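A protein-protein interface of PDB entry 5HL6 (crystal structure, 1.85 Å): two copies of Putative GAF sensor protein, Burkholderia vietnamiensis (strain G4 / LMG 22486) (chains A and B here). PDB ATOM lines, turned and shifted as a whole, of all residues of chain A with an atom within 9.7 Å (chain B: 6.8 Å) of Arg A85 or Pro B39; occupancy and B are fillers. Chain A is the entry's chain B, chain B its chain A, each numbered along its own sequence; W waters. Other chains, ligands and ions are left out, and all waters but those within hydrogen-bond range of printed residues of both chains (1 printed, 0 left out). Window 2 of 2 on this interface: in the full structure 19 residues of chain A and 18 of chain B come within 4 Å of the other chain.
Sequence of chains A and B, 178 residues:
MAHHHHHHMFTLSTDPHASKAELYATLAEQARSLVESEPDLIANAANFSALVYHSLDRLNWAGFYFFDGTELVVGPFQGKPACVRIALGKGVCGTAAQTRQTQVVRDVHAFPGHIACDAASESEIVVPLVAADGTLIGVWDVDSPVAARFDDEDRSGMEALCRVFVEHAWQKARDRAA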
ATOM      1  N   PHE A  64      28.956 -21.629  -7.473  1.00  0.00           N
ATOM      2  CA  PHE A  64      28.787 -21.018  -6.162  1.00  0.00           C
ATOM      3  C   PHE A  64      28.092 -21.960  -5.187  1.00  0.00           C
ATOM      4  O   PHE A  64      27.206 -22.723  -5.570  1.00  0.00           O
ATOM      5  CB  PHE A  64      27.925 -19.752  -6.271  1.00  0.00           C
ATOM      6  CG  PHE A  64      28.565 -18.642  -7.044  1.00  0.00           C
ATOM      7  CD1 PHE A  64      29.381 -17.721  -6.404  1.00  0.00           C
ATOM      8  CD2 PHE A  64      28.331 -18.504  -8.402  1.00  0.00           C
ATOM      9  CE1 PHE A  64      29.974 -16.683  -7.104  1.00  0.00           C
ATOM     10  CE2 PHE A  64      28.904 -17.461  -9.112  1.00  0.00           C
ATOM     11  CZ  PHE A  64      29.737 -16.549  -8.457  1.00  0.00           C
ATOM     12  N   TYR A  65      28.472 -21.873  -3.912  1.00  0.00           N
ATOM     13  CA  TYR A  65      27.615 -22.284  -2.804  1.00  0.00           C
ATOM     14  C   TYR A  65      27.332 -21.033  -1.991  1.00  0.00           C
ATOM     15  O   TYR A  65      28.250 -20.249  -1.712  1.00  0.00           O
ATOM     16  CB  TYR A  65      28.246 -23.370  -1.906  1.00  0.00           C
ATOM     17  CG  TYR A  65      28.434 -24.710  -2.574  1.00  0.00           C
ATOM     18  CD1 TYR A  65      27.554 -25.758  -2.340  1.00  0.00           C
ATOM     19  CD2 TYR A  65      29.506 -24.935  -3.428  1.00  0.00           C
ATOM     20  CE1 TYR A  65      27.729 -26.988  -2.953  1.00  0.00           C
ATOM     21  CE2 TYR A  65      29.690 -26.146  -4.044  1.00  0.00           C
ATOM     22  CZ  TYR A  65      28.801 -27.174  -3.816  1.00  0.00           C
ATOM     23  OH  TYR A  65      28.991 -28.387  -4.444  1.00  0.00           O
ATOM     24  N   PHE A  66      26.070 -20.823  -1.639  1.00  0.00           N
ATOM     25  CA  PHE A  66      25.676 -19.637  -0.892  1.00  0.00           C
ATOM     26  C   PHE A  66      25.319 -20.021   0.538  1.00  0.00           C
ATOM     27  O   PHE A  66      24.596 -20.997   0.769  1.00  0.00           O
ATOM     28  CB  PHE A  66      24.511 -18.920  -1.586  1.00  0.00           C
ATOM     29  CG  PHE A  66      24.922 -18.228  -2.856  1.00  0.00           C
ATOM     30  CD1 PHE A  66      25.850 -17.194  -2.819  1.00  0.00           C
ATOM     31  CD2 PHE A  66      24.402 -18.613  -4.080  1.00  0.00           C
ATOM     32  CE1 PHE A  66      26.259 -16.553  -3.978  1.00  0.00           C
ATOM     33  CE2 PHE A  66      24.801 -17.967  -5.253  1.00  0.00           C
ATOM     34  CZ  PHE A  66      25.729 -16.935  -5.194  1.00  0.00           C
ATOM     35  N   PHE A  67      25.843 -19.253   1.487  1.00  0.00           N
ATOM     36  CA  PHE A  67      25.544 -19.440   2.898  1.00  0.00           C
ATOM     37  C   PHE A  67      24.111 -19.009   3.187  1.00  0.00           C
ATOM     38  O   PHE A  67      23.728 -17.870   2.894  1.00  0.00           O
ATOM     39  CB  PHE A  67      26.533 -18.631   3.730  1.00  0.00           C
ATOM     40  CG  PHE A  67      26.471 -18.916   5.192  1.00  0.00           C
ATOM     41  CD1 PHE A  67      26.703 -20.201   5.671  1.00  0.00           C
ATOM     42  CD2 PHE A  67      26.216 -17.902   6.096  1.00  0.00           C
ATOM     43  CE1 PHE A  67      26.659 -20.467   7.038  1.00  0.00           C
ATOM     44  CE2 PHE A  67      26.177 -18.160   7.460  1.00  0.00           C
ATOM     45  CZ  PHE A  67      26.394 -19.447   7.929  1.00  0.00           C
ATOM     46  N   ASP A  68      23.310 -19.914   3.759  1.00  0.00           N
ATOM     47  CA  ASP A  68      21.917 -19.607   4.058  1.00  0.00           C
ATOM     48  C   ASP A  68      21.715 -19.172   5.506  1.00  0.00           C
ATOM     49  O   ASP A  68      20.585 -19.174   5.999  1.00  0.00           O
ATOM     50  CB  ASP A  68      21.017 -20.798   3.713  1.00  0.00           C
ATOM     51  CG  ASP A  68      21.123 -21.954   4.709  1.00  0.00           C
ATOM     52  OD1 ASP A  68      22.024 -21.958   5.579  1.00  0.00           O
ATOM     53  OD2 ASP A  68      20.287 -22.876   4.606  1.00  0.00           O
ATOM     54  N   GLY A  69      22.782 -18.777   6.183  1.00  0.00           N
ATOM     55  CA  GLY A  69      22.721 -18.457   7.585  1.00  0.00           C
ATOM     56  C   GLY A  69      23.076 -19.606   8.497  1.00  0.00           C
ATOM     57  O   GLY A  69      23.420 -19.375   9.661  1.00  0.00           O
ATOM     58  N   THR A  70      23.008 -20.837   7.997  1.00  0.00           N
ATOM     59  CA  THR A  70      23.379 -22.018   8.767  1.00  0.00           C
ATOM     60  C   THR A  70      24.445 -22.842   8.068  1.00  0.00           C
ATOM     61  O   THR A  70      25.425 -23.253   8.703  1.00  0.00           O
ATOM     62  CB  THR A  70      22.131 -22.877   9.026  1.00  0.00           C
ATOM     63  OG1 THR A  70      21.208 -22.140   9.836  1.00  0.00           O
ATOM     64  CG2 THR A  70      22.502 -24.179   9.721  1.00  0.00           C
ATOM     65  N   GLU A  71      24.283 -23.096   6.768  1.00  0.00           N
ATOM     66  CA  GLU A  71      25.224 -23.912   6.022  1.00  0.00           C
ATOM     67  C   GLU A  71      25.259 -23.426   4.583  1.00  0.00           C
ATOM     68  O   GLU A  71      24.507 -22.527   4.192  1.00  0.00           O
ATOM     69  CB  GLU A  71      24.848 -25.398   6.104  1.00  0.00           C
ATOM     70  CG  GLU A  71      23.476 -25.722   5.531  1.00  0.00           C
ATOM     71  CD  GLU A  71      23.112 -27.189   5.704  1.00  0.00           C
ATOM     72  OE1 GLU A  71      23.989 -27.987   6.106  1.00  0.00           O
ATOM     73  OE2 GLU A  71      21.942 -27.536   5.442  1.00  0.00           O
ATOM     74  N   LEU A  72      26.141 -24.036   3.790  1.00  0.00           N
ATOM     75  CA  LEU A  72      26.221 -23.757   2.358  1.00  0.00           C
ATOM     76  C   LEU A  72      25.150 -24.522   1.576  1.00  0.00           C
ATOM     77  O   LEU A  72      24.841 -25.682   1.881  1.00  0.00           O
ATOM     78  CB  LEU A  72      27.607 -24.129   1.827  1.00  0.00           C
ATOM     79  CG  LEU A  72      28.785 -23.359   2.427  1.00  0.00           C
ATOM     80  CD1 LEU A  72      30.099 -23.941   1.942  1.00  0.00           C
ATOM     81  CD2 LEU A  72      28.672 -21.916   1.985  1.00  0.00           C
ATOM     82  N   VAL A  73      24.592 -23.856   0.559  1.00  0.00           N
ATOM     83  CA  VAL A  73      23.566 -24.412  -0.324  1.00  0.00           C
ATOM     84  C   VAL A  73      23.975 -24.079  -1.753  1.00  0.00           C
ATOM     85  O   VAL A  73      24.318 -22.929  -2.044  1.00  0.00           O
ATOM     86  CB  VAL A  73      22.167 -23.834  -0.026  1.00  0.00           C
ATOM     87  CG1 VAL A  73      21.108 -24.544  -0.886  1.00  0.00           C
ATOM     88  CG2 VAL A  73      21.820 -23.929   1.471  1.00  0.00           C
ATOM     89  N   VAL A  74      23.969 -25.082  -2.639  1.00  0.00           N
ATOM     90  CA  VAL A  74      24.536 -24.869  -3.967  1.00  0.00           C
ATOM     91  C   VAL A  74      23.717 -23.822  -4.714  1.00  0.00           C
ATOM     92  O   VAL A  74      22.482 -23.783  -4.614  1.00  0.00           O
ATOM     93  CB  VAL A  74      24.612 -26.188  -4.755  1.00  0.00           C
ATOM     94  CG1 VAL A  74      23.214 -26.662  -5.206  1.00  0.00           C
ATOM     95  CG2 VAL A  74      25.535 -26.033  -5.957  1.00  0.00           C
ATOM     96  N   GLY A  75      24.414 -22.946  -5.441  1.00  0.00           N
ATOM     97  CA  GLY A  75      23.793 -21.952  -6.303  1.00  0.00           C
ATOM     98  C   GLY A  75      24.029 -22.318  -7.755  1.00  0.00           C
ATOM     99  O   GLY A  75      24.215 -23.493  -8.074  1.00  0.00           O
ATOM    100  N   ALA A  82      26.599 -31.944  -7.981  1.00  0.00           N
ATOM    101  CA  ALA A  82      27.627 -32.174  -6.970  1.00  0.00           C
ATOM    102  C   ALA A  82      26.999 -32.233  -5.581  1.00  0.00           C
ATOM    103  O   ALA A  82      25.969 -32.882  -5.391  1.00  0.00           O
ATOM    104  CB  ALA A  82      28.702 -31.085  -7.033  1.00  0.00           C
ATOM    105  N   CYS A  83      27.601 -31.571  -4.600  1.00  0.00           N
ATOM    106  CA  CYS A  83      26.926 -31.429  -3.320  1.00  0.00           C
ATOM    107  C   CYS A  83      25.780 -30.432  -3.434  1.00  0.00           C
ATOM    108  O   CYS A  83      25.827 -29.493  -4.226  1.00  0.00           O
ATOM    109  CB  CYS A  83      27.897 -30.954  -2.242  1.00  0.00           C
ATOM    110  SG  CYS A  83      29.148 -32.159  -1.782  1.00  0.00           S
ATOM    111  N   VAL A  84      24.747 -30.641  -2.628  1.00  0.00           N
ATOM    112  CA  VAL A  84      23.632 -29.703  -2.527  1.00  0.00           C
ATOM    113  C   VAL A  84      23.752 -28.846  -1.275  1.00  0.00           C
ATOM    114  O   VAL A  84      23.677 -27.618  -1.344  1.00  0.00           O
ATOM    115  CB  VAL A  84      22.287 -30.460  -2.568  1.00  0.00           C
ATOM    116  CG1 VAL A  84      21.129 -29.481  -2.638  1.00  0.00           C
ATOM    117  CG2 VAL A  84      22.254 -31.415  -3.757  1.00  0.00           C
ATOM    118  N   ARG A  85      23.960 -29.478  -0.123  1.00  0.00           N
ATOM    119  CA  ARG A  85      24.179 -28.777   1.135  1.00  0.00           C
ATOM    120  C   ARG A  85      25.498 -29.214   1.753  1.00  0.00           C
ATOM    121  O   ARG A  85      25.826 -30.407   1.765  1.00  0.00           O
ATOM    122  CB  ARG A  85      23.029 -29.025   2.114  1.00  0.00           C
ATOM    123  CG  ARG A  85      21.790 -28.257   1.715  1.00  0.00           C
ATOM    124  CD  ARG A  85      20.574 -28.513   2.582  1.00  0.00           C
ATOM    125  NE  ARG A  85      19.522 -27.629   2.100  1.00  0.00           N
ATOM    126  CZ  ARG A  85      19.329 -26.397   2.560  1.00  0.00           C
ATOM    127  NH1 ARG A  85      20.086 -25.946   3.553  1.00  0.00           N
ATOM    128  NH2 ARG A  85      18.375 -25.625   2.039  1.00  0.00           N
ATOM    129  N   ILE A  86      26.249 -28.243   2.272  1.00  0.00           N
ATOM    130  CA  ILE A  86      27.542 -28.502   2.902  1.00  0.00           C
ATOM    131  C   ILE A  86      27.591 -27.760   4.235  1.00  0.00           C
ATOM    132  O   ILE A  86      27.432 -26.533   4.275  1.00  0.00           O
ATOM    133  CB  ILE A  86      28.716 -28.079   2.005  1.00  0.00           C
ATOM    134  CG1 ILE A  86      28.679 -28.836   0.680  1.00  0.00           C
ATOM    135  CG2 ILE A  86      30.046 -28.339   2.694  1.00  0.00           C
ATOM    136  CD1 ILE A  86      29.664 -28.320  -0.330  1.00  0.00           C
ATOM    137  N   ALA A  87      27.821 -28.503   5.321  1.00  0.00           N
ATOM    138  CA  ALA A  87      27.950 -27.898   6.635  1.00  0.00           C
ATOM    139  C   ALA A  87      29.269 -27.142   6.743  1.00  0.00           C
ATOM    140  O   ALA A  87      30.267 -27.499   6.111  1.00  0.00           O
ATOM    141  CB  ALA A  87      27.877 -28.964   7.729  1.00  0.00           C
ATOM    142  N   LEU A  88      29.261 -26.080   7.548  1.00  0.00           N
ATOM    143  CA  LEU A  88      30.499 -25.390   7.886  1.00  0.00           C
ATOM    144  C   LEU A  88      31.527 -26.388   8.403  1.00  0.00           C
ATOM    145  O   LEU A  88      31.211 -27.253   9.225  1.00  0.00           O
ATOM    146  CB  LEU A  88      30.229 -24.308   8.933  1.00  0.00           C
ATOM    147  CG  LEU A  88      29.538 -23.024   8.429  1.00  0.00           C
ATOM    148  CD1 LEU A  88      29.327 -22.036   9.559  1.00  0.00           C
ATOM    149  CD2 LEU A  88      30.304 -22.367   7.276  1.00  0.00           C
ATOM    150  N   LYS A  90      32.952 -28.843   6.762  1.00  0.00           N
ATOM    151  CA  LYS A  90      32.933 -30.169   6.153  1.00  0.00           C
ATOM    152  C   LYS A  90      33.487 -30.076   4.736  1.00  0.00           C
ATOM    153  O   LYS A  90      32.969 -29.314   3.911  1.00  0.00           O
ATOM    154  CB  LYS A  90      31.521 -30.755   6.150  1.00  0.00           C
ATOM    155  N   GLY A  91      34.552 -30.834   4.465  1.00  0.00           N
ATOM    156  CA  GLY A  91      35.134 -30.867   3.133  1.00  0.00           C
ATOM    157  C   GLY A  91      35.862 -29.581   2.772  1.00  0.00           C
ATOM    158  O   GLY A  91      35.983 -28.650   3.563  1.00  0.00           O
ATOM    159  N   CYS A  93      35.053 -27.209   0.589  1.00  0.00           N
ATOM    160  CA  CYS A  93      34.175 -26.040   0.538  1.00  0.00           C
ATOM    161  C   CYS A  93      33.734 -25.594   1.926  1.00  0.00           C
ATOM    162  O   CYS A  93      33.709 -24.389   2.222  1.00  0.00           O
ATOM    163  CB  CYS A  93      32.949 -26.341  -0.327  1.00  0.00           C
ATOM    164  SG  CYS A  93      33.302 -26.382  -2.084  1.00  0.00           S
ATOM    165  N   GLY A  94      33.340 -26.542   2.781  1.00  0.00           N
ATOM    166  CA  GLY A  94      32.954 -26.180   4.134  1.00  0.00           C
ATOM    167  C   GLY A  94      34.124 -25.651   4.937  1.00  0.00           C
ATOM    168  O   GLY A  94      33.959 -24.742   5.760  1.00  0.00           O
ATOM    169  N   ILE A 115      36.944 -35.821   0.497  1.00  0.00           N
ATOM    170  CA  ILE A 115      35.535 -36.073   0.779  1.00  0.00           C
ATOM    171  C   ILE A 115      34.646 -35.134  -0.040  1.00  0.00           C
ATOM    172  O   ILE A 115      34.601 -33.934   0.236  1.00  0.00           O
ATOM    173  CB  ILE A 115      35.240 -35.929   2.287  1.00  0.00           C
ATOM    174  N   ALA A 116      33.963 -35.685  -1.054  1.00  0.00           N
ATOM    175  CA  ALA A 116      33.007 -34.948  -1.881  1.00  0.00           C
ATOM    176  C   ALA A 116      33.735 -33.921  -2.755  1.00  0.00           C
ATOM    177  O   ALA A 116      34.916 -33.651  -2.515  1.00  0.00           O
ATOM    178  CB  ALA A 116      31.942 -34.307  -0.981  1.00  0.00           C
ATOM    179  N   CYS A 117      33.097 -33.359  -3.790  1.00  0.00           N
ATOM    180  CA  CYS A 117      31.735 -33.647  -4.249  1.00  0.00           C
ATOM    181  C   CYS A 117      31.743 -34.224  -5.659  1.00  0.00           C
ATOM    182  O   CYS A 117      31.299 -35.348  -5.889  1.00  0.00           O
ATOM    183  CB  CYS A 117      30.881 -32.375  -4.237  1.00  0.00           C
ATOM    184  SG  CYS A 117      30.842 -31.480  -2.671  1.00  0.00           S
ATOM    185  N   VAL B  35      14.722 -32.985  -6.265  1.00  0.00           N
ATOM    186  CA  VAL B  35      14.191 -31.695  -5.821  1.00  0.00           C
ATOM    187  C   VAL B  35      13.259 -31.828  -4.614  1.00  0.00           C
ATOM    188  O   VAL B  35      13.112 -30.867  -3.845  1.00  0.00           O
ATOM    189  CB  VAL B  35      13.487 -30.955  -6.978  1.00  0.00           C
ATOM    190  CG1 VAL B  35      14.399 -30.889  -8.180  1.00  0.00           C
ATOM    191  CG2 VAL B  35      12.179 -31.645  -7.334  1.00  0.00           C
ATOM    192  N   GLU B  36      12.634 -32.997  -4.423  1.00  0.00           N
ATOM    193  CA  GLU B  36      11.731 -33.185  -3.293  1.00  0.00           C
ATOM    194  C   GLU B  36      12.476 -33.118  -1.965  1.00  0.00           C
ATOM    195  O   GLU B  36      11.903 -32.700  -0.953  1.00  0.00           O
ATOM    196  CB  GLU B  36      10.999 -34.528  -3.417  1.00  0.00           C
ATOM    197  N   SER B  37      13.748 -33.515  -1.956  1.00  0.00           N
ATOM    198  CA  SER B  37      14.563 -33.549  -0.752  1.00  0.00           C
ATOM    199  C   SER B  37      15.289 -32.231  -0.485  1.00  0.00           C
ATOM    200  O   SER B  37      16.241 -32.214   0.306  1.00  0.00           O
ATOM    201  CB  SER B  37      15.581 -34.689  -0.850  1.00  0.00           C
ATOM    202  OG  SER B  37      16.356 -34.565  -2.037  1.00  0.00           O
ATOM    203  N   GLU B  38      14.865 -31.128  -1.122  1.00  0.00           N
ATOM    204  CA  GLU B  38      15.593 -29.865  -1.021  1.00  0.00           C
ATOM    205  C   GLU B  38      14.675 -28.647  -1.125  1.00  0.00           C
ATOM    206  O   GLU B  38      13.990 -28.465  -2.140  1.00  0.00           O
ATOM    207  CB  GLU B  38      16.669 -29.786  -2.106  1.00  0.00           C
ATOM    208  CG  GLU B  38      17.267 -28.389  -2.235  1.00  0.00           C
ATOM    209  CD  GLU B  38      17.876 -27.921  -0.934  1.00  0.00           C
ATOM    210  OE1 GLU B  38      18.533 -28.749  -0.263  1.00  0.00           O
ATOM    211  OE2 GLU B  38      17.684 -26.742  -0.567  1.00  0.00           O
ATOM    212  N   PRO B  39      14.656 -27.774  -0.108  1.00  0.00           N
ATOM    213  CA  PRO B  39      13.749 -26.614  -0.140  1.00  0.00           C
ATOM    214  C   PRO B  39      14.142 -25.478  -1.084  1.00  0.00           C
ATOM    215  O   PRO B  39      13.263 -24.752  -1.555  1.00  0.00           O
ATOM    216  CB  PRO B  39      13.755 -26.132   1.319  1.00  0.00           C
ATOM    217  CG  PRO B  39      15.024 -26.659   1.901  1.00  0.00           C
ATOM    218  CD  PRO B  39      15.264 -27.972   1.219  1.00  0.00           C
ATOM    219  N   ASP B  40      15.434 -25.291  -1.360  1.00  0.00           N
ATOM    220  CA  ASP B  40      15.913 -24.076  -2.021  1.00  0.00           C
ATOM    221  C   ASP B  40      15.657 -24.138  -3.525  1.00  0.00           C
ATOM    222  O   ASP B  40      16.108 -25.068  -4.203  1.00  0.00           O
ATOM    223  CB  ASP B  40      17.402 -23.872  -1.744  1.00  0.00           C
ATOM    224  CG  ASP B  40      17.924 -22.530  -2.247  1.00  0.00           C
ATOM    225  OD1 ASP B  40      18.253 -22.421  -3.447  1.00  0.00           O
ATOM    226  OD2 ASP B  40      18.026 -21.588  -1.431  1.00  0.00           O
ATOM    227  N   LEU B  41      14.956 -23.133  -4.048  1.00  0.00           N
ATOM    228  CA  LEU B  41      14.560 -23.157  -5.453  1.00  0.00           C
ATOM    229  C   LEU B  41      15.760 -23.009  -6.380  1.00  0.00           C
ATOM    230  O   LEU B  41      15.782 -23.586  -7.473  1.00  0.00           O
ATOM    231  CB  LEU B  41      13.539 -22.047  -5.730  1.00  0.00           C
ATOM    232  CG  LEU B  41      13.110 -21.955  -7.197  1.00  0.00           C
ATOM    233  CD1 LEU B  41      12.342 -23.218  -7.630  1.00  0.00           C
ATOM    234  CD2 LEU B  41      12.300 -20.687  -7.463  1.00  0.00           C
ATOM    235  N   ILE B  42      16.745 -22.196  -5.986  1.00  0.00           N
ATOM    236  CA  ILE B  42      17.916 -21.979  -6.833  1.00  0.00           C
ATOM    237  C   ILE B  42      18.738 -23.255  -6.920  1.00  0.00           C
ATOM    238  O   ILE B  42      19.205 -23.646  -7.996  1.00  0.00           O
ATOM    239  CB  ILE B  42      18.765 -20.815  -6.289  1.00  0.00           C
ATOM    240  CG1 ILE B  42      17.954 -19.521  -6.278  1.00  0.00           C
ATOM    241  CG2 ILE B  42      20.024 -20.645  -7.126  1.00  0.00           C
ATOM    242  CD1 ILE B  42      17.461 -19.113  -7.652  1.00  0.00           C
ATOM    243  N   ALA B  43      18.946 -23.906  -5.774  1.00  0.00           N
ATOM    244  CA  ALA B  43      19.607 -25.201  -5.770  1.00  0.00           C
ATOM    245  C   ALA B  43      18.883 -26.173  -6.692  1.00  0.00           C
ATOM    246  O   ALA B  43      19.510 -26.851  -7.517  1.00  0.00           O
ATOM    247  CB  ALA B  43      19.669 -25.751  -4.344  1.00  0.00           C
ATOM    248  N   ASN B  44      17.554 -26.242  -6.579  1.00  0.00           N
ATOM    249  CA  ASN B  44      16.798 -27.187  -7.401  1.00  0.00           C
ATOM    250  C   ASN B  44      16.892 -26.839  -8.882  1.00  0.00           C
ATOM    251  O   ASN B  44      17.036 -27.733  -9.728  1.00  0.00           O
ATOM    252  CB  ASN B  44      15.339 -27.249  -6.945  1.00  0.00           C
ATOM    253  CG  ASN B  44      15.165 -28.026  -5.649  1.00  0.00           C
ATOM    254  OD1 ASN B  44      15.959 -28.917  -5.344  1.00  0.00           O
ATOM    255  ND2 ASN B  44      14.124 -27.698  -4.883  1.00  0.00           N
ATOM    256  N   ALA B 169       9.345 -28.352  -6.829  1.00  0.00           N
ATOM    257  CA  ALA B 169      10.363 -27.358  -6.510  1.00  0.00           C
ATOM    258  C   ALA B 169       9.756 -25.967  -6.405  1.00  0.00           C
ATOM    259  O   ALA B 169       9.862 -25.332  -5.351  1.00  0.00           O
ATOM    260  CB  ALA B 169      11.495 -27.372  -7.548  1.00  0.00           C
ATOM    261  N   LYS B 172       6.336 -25.900  -4.142  1.00  0.00           N
ATOM    262  CA  LYS B 172       6.675 -26.112  -2.739  1.00  0.00           C
ATOM    263  C   LYS B 172       7.249 -24.845  -2.108  1.00  0.00           C
ATOM    264  O   LYS B 172       6.774 -24.392  -1.060  1.00  0.00           O
ATOM    265  CB  LYS B 172       7.662 -27.272  -2.619  1.00  0.00           C
ATOM    266  CG  LYS B 172       8.193 -27.485  -1.215  1.00  0.00           C
ATOM    267  CD  LYS B 172       9.230 -28.591  -1.191  1.00  0.00           C
ATOM    268  CE  LYS B 172      10.419 -28.263  -2.080  1.00  0.00           C
ATOM    269  NZ  LYS B 172      11.327 -29.447  -2.176  1.00  0.00           N
ATOM    270  N   ALA B 173       8.273 -24.259  -2.735  1.00  0.00           N
ATOM    271  CA  ALA B 173       8.926 -23.086  -2.155  1.00  0.00           C
ATOM    272  C   ALA B 173       7.966 -21.911  -2.043  1.00  0.00           C
ATOM    273  O   ALA B 173       8.056 -21.115  -1.102  1.00  0.00           O
ATOM    274  CB  ALA B 173      10.148 -22.700  -2.987  1.00  0.00           C
HETATM  275  O   HOH W   1      21.005 -21.732  -3.635  1.00  0.00           O
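No position is printed for both chains. Of the 6 pairs that touch across the chains among the printed residues, none has its exchanged pair printed and touching as well.
The side-chain carboxylate of Glu B38 is in salt-bridge range of the guanidinium group of Arg A85 (2.8 Å).
Water W1 lies within hydrogen-bond range of the backbone carbonyl oxygen (O) of Val A74 and the side-chain carboxylate (OD1) of Asp B40.
Hydrophobic or aromatic side chains of chain A that line the printed part of chain B: Val A73, Val A74 and Val A84. Along chain A the printed residues that touch a printed residue of chain B span positions 73 to 85. Among the printed residues, 6 pairs touch across the chains.
Among the printed residues, pairs that only touch across the chains: Val A73 with Asp B40, Val A73 with Ala B43, Val A74 with Ala B43, Val A84 with Glu B38 and Arg A85 with Pro B39.
Pro B39 touches one residue of chain A. Of chain A, only Val A73 (3.9 Å) comes within 4 Å of Asp B40. Of the printed residues of chain B, Val A74 touches Ala B43. Printed residues of chain A within 4 Å of Ala B43: Val A73 and Val A74. The nearest residue of chain B that does not touch Arg A85 is Asp B40 (4.3 Å).
The backbone carbonyl oxygen of Val A84 sits at hydrogen-bond distance from the backbone NH of Val A74, at 2.9 Å. ND2 of Asn B44 lies within hydrogen-bond range of O of Glu B38 (2.9 Å). The side-chain carboxylate (OD1) of Asp B40 is in hydrogen-bond range of the backbone NH (N) of Ile B42 (3.0 Å). The side-chain sulfur (SG) of Cys A83 forms a disulfide with the side-chain sulfur (SG) of Cys A117, 2.0 Å away. The backbone carbonyl oxygen of Asp B40 is in hydrogen-bond range of the side-chain amide nitrogen of Asn B44 (3.4 Å). The side-chain carboxylate of Asp A68 lies within salt-bridge range of the guanidinium group of Arg A85 (3.3 Å).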
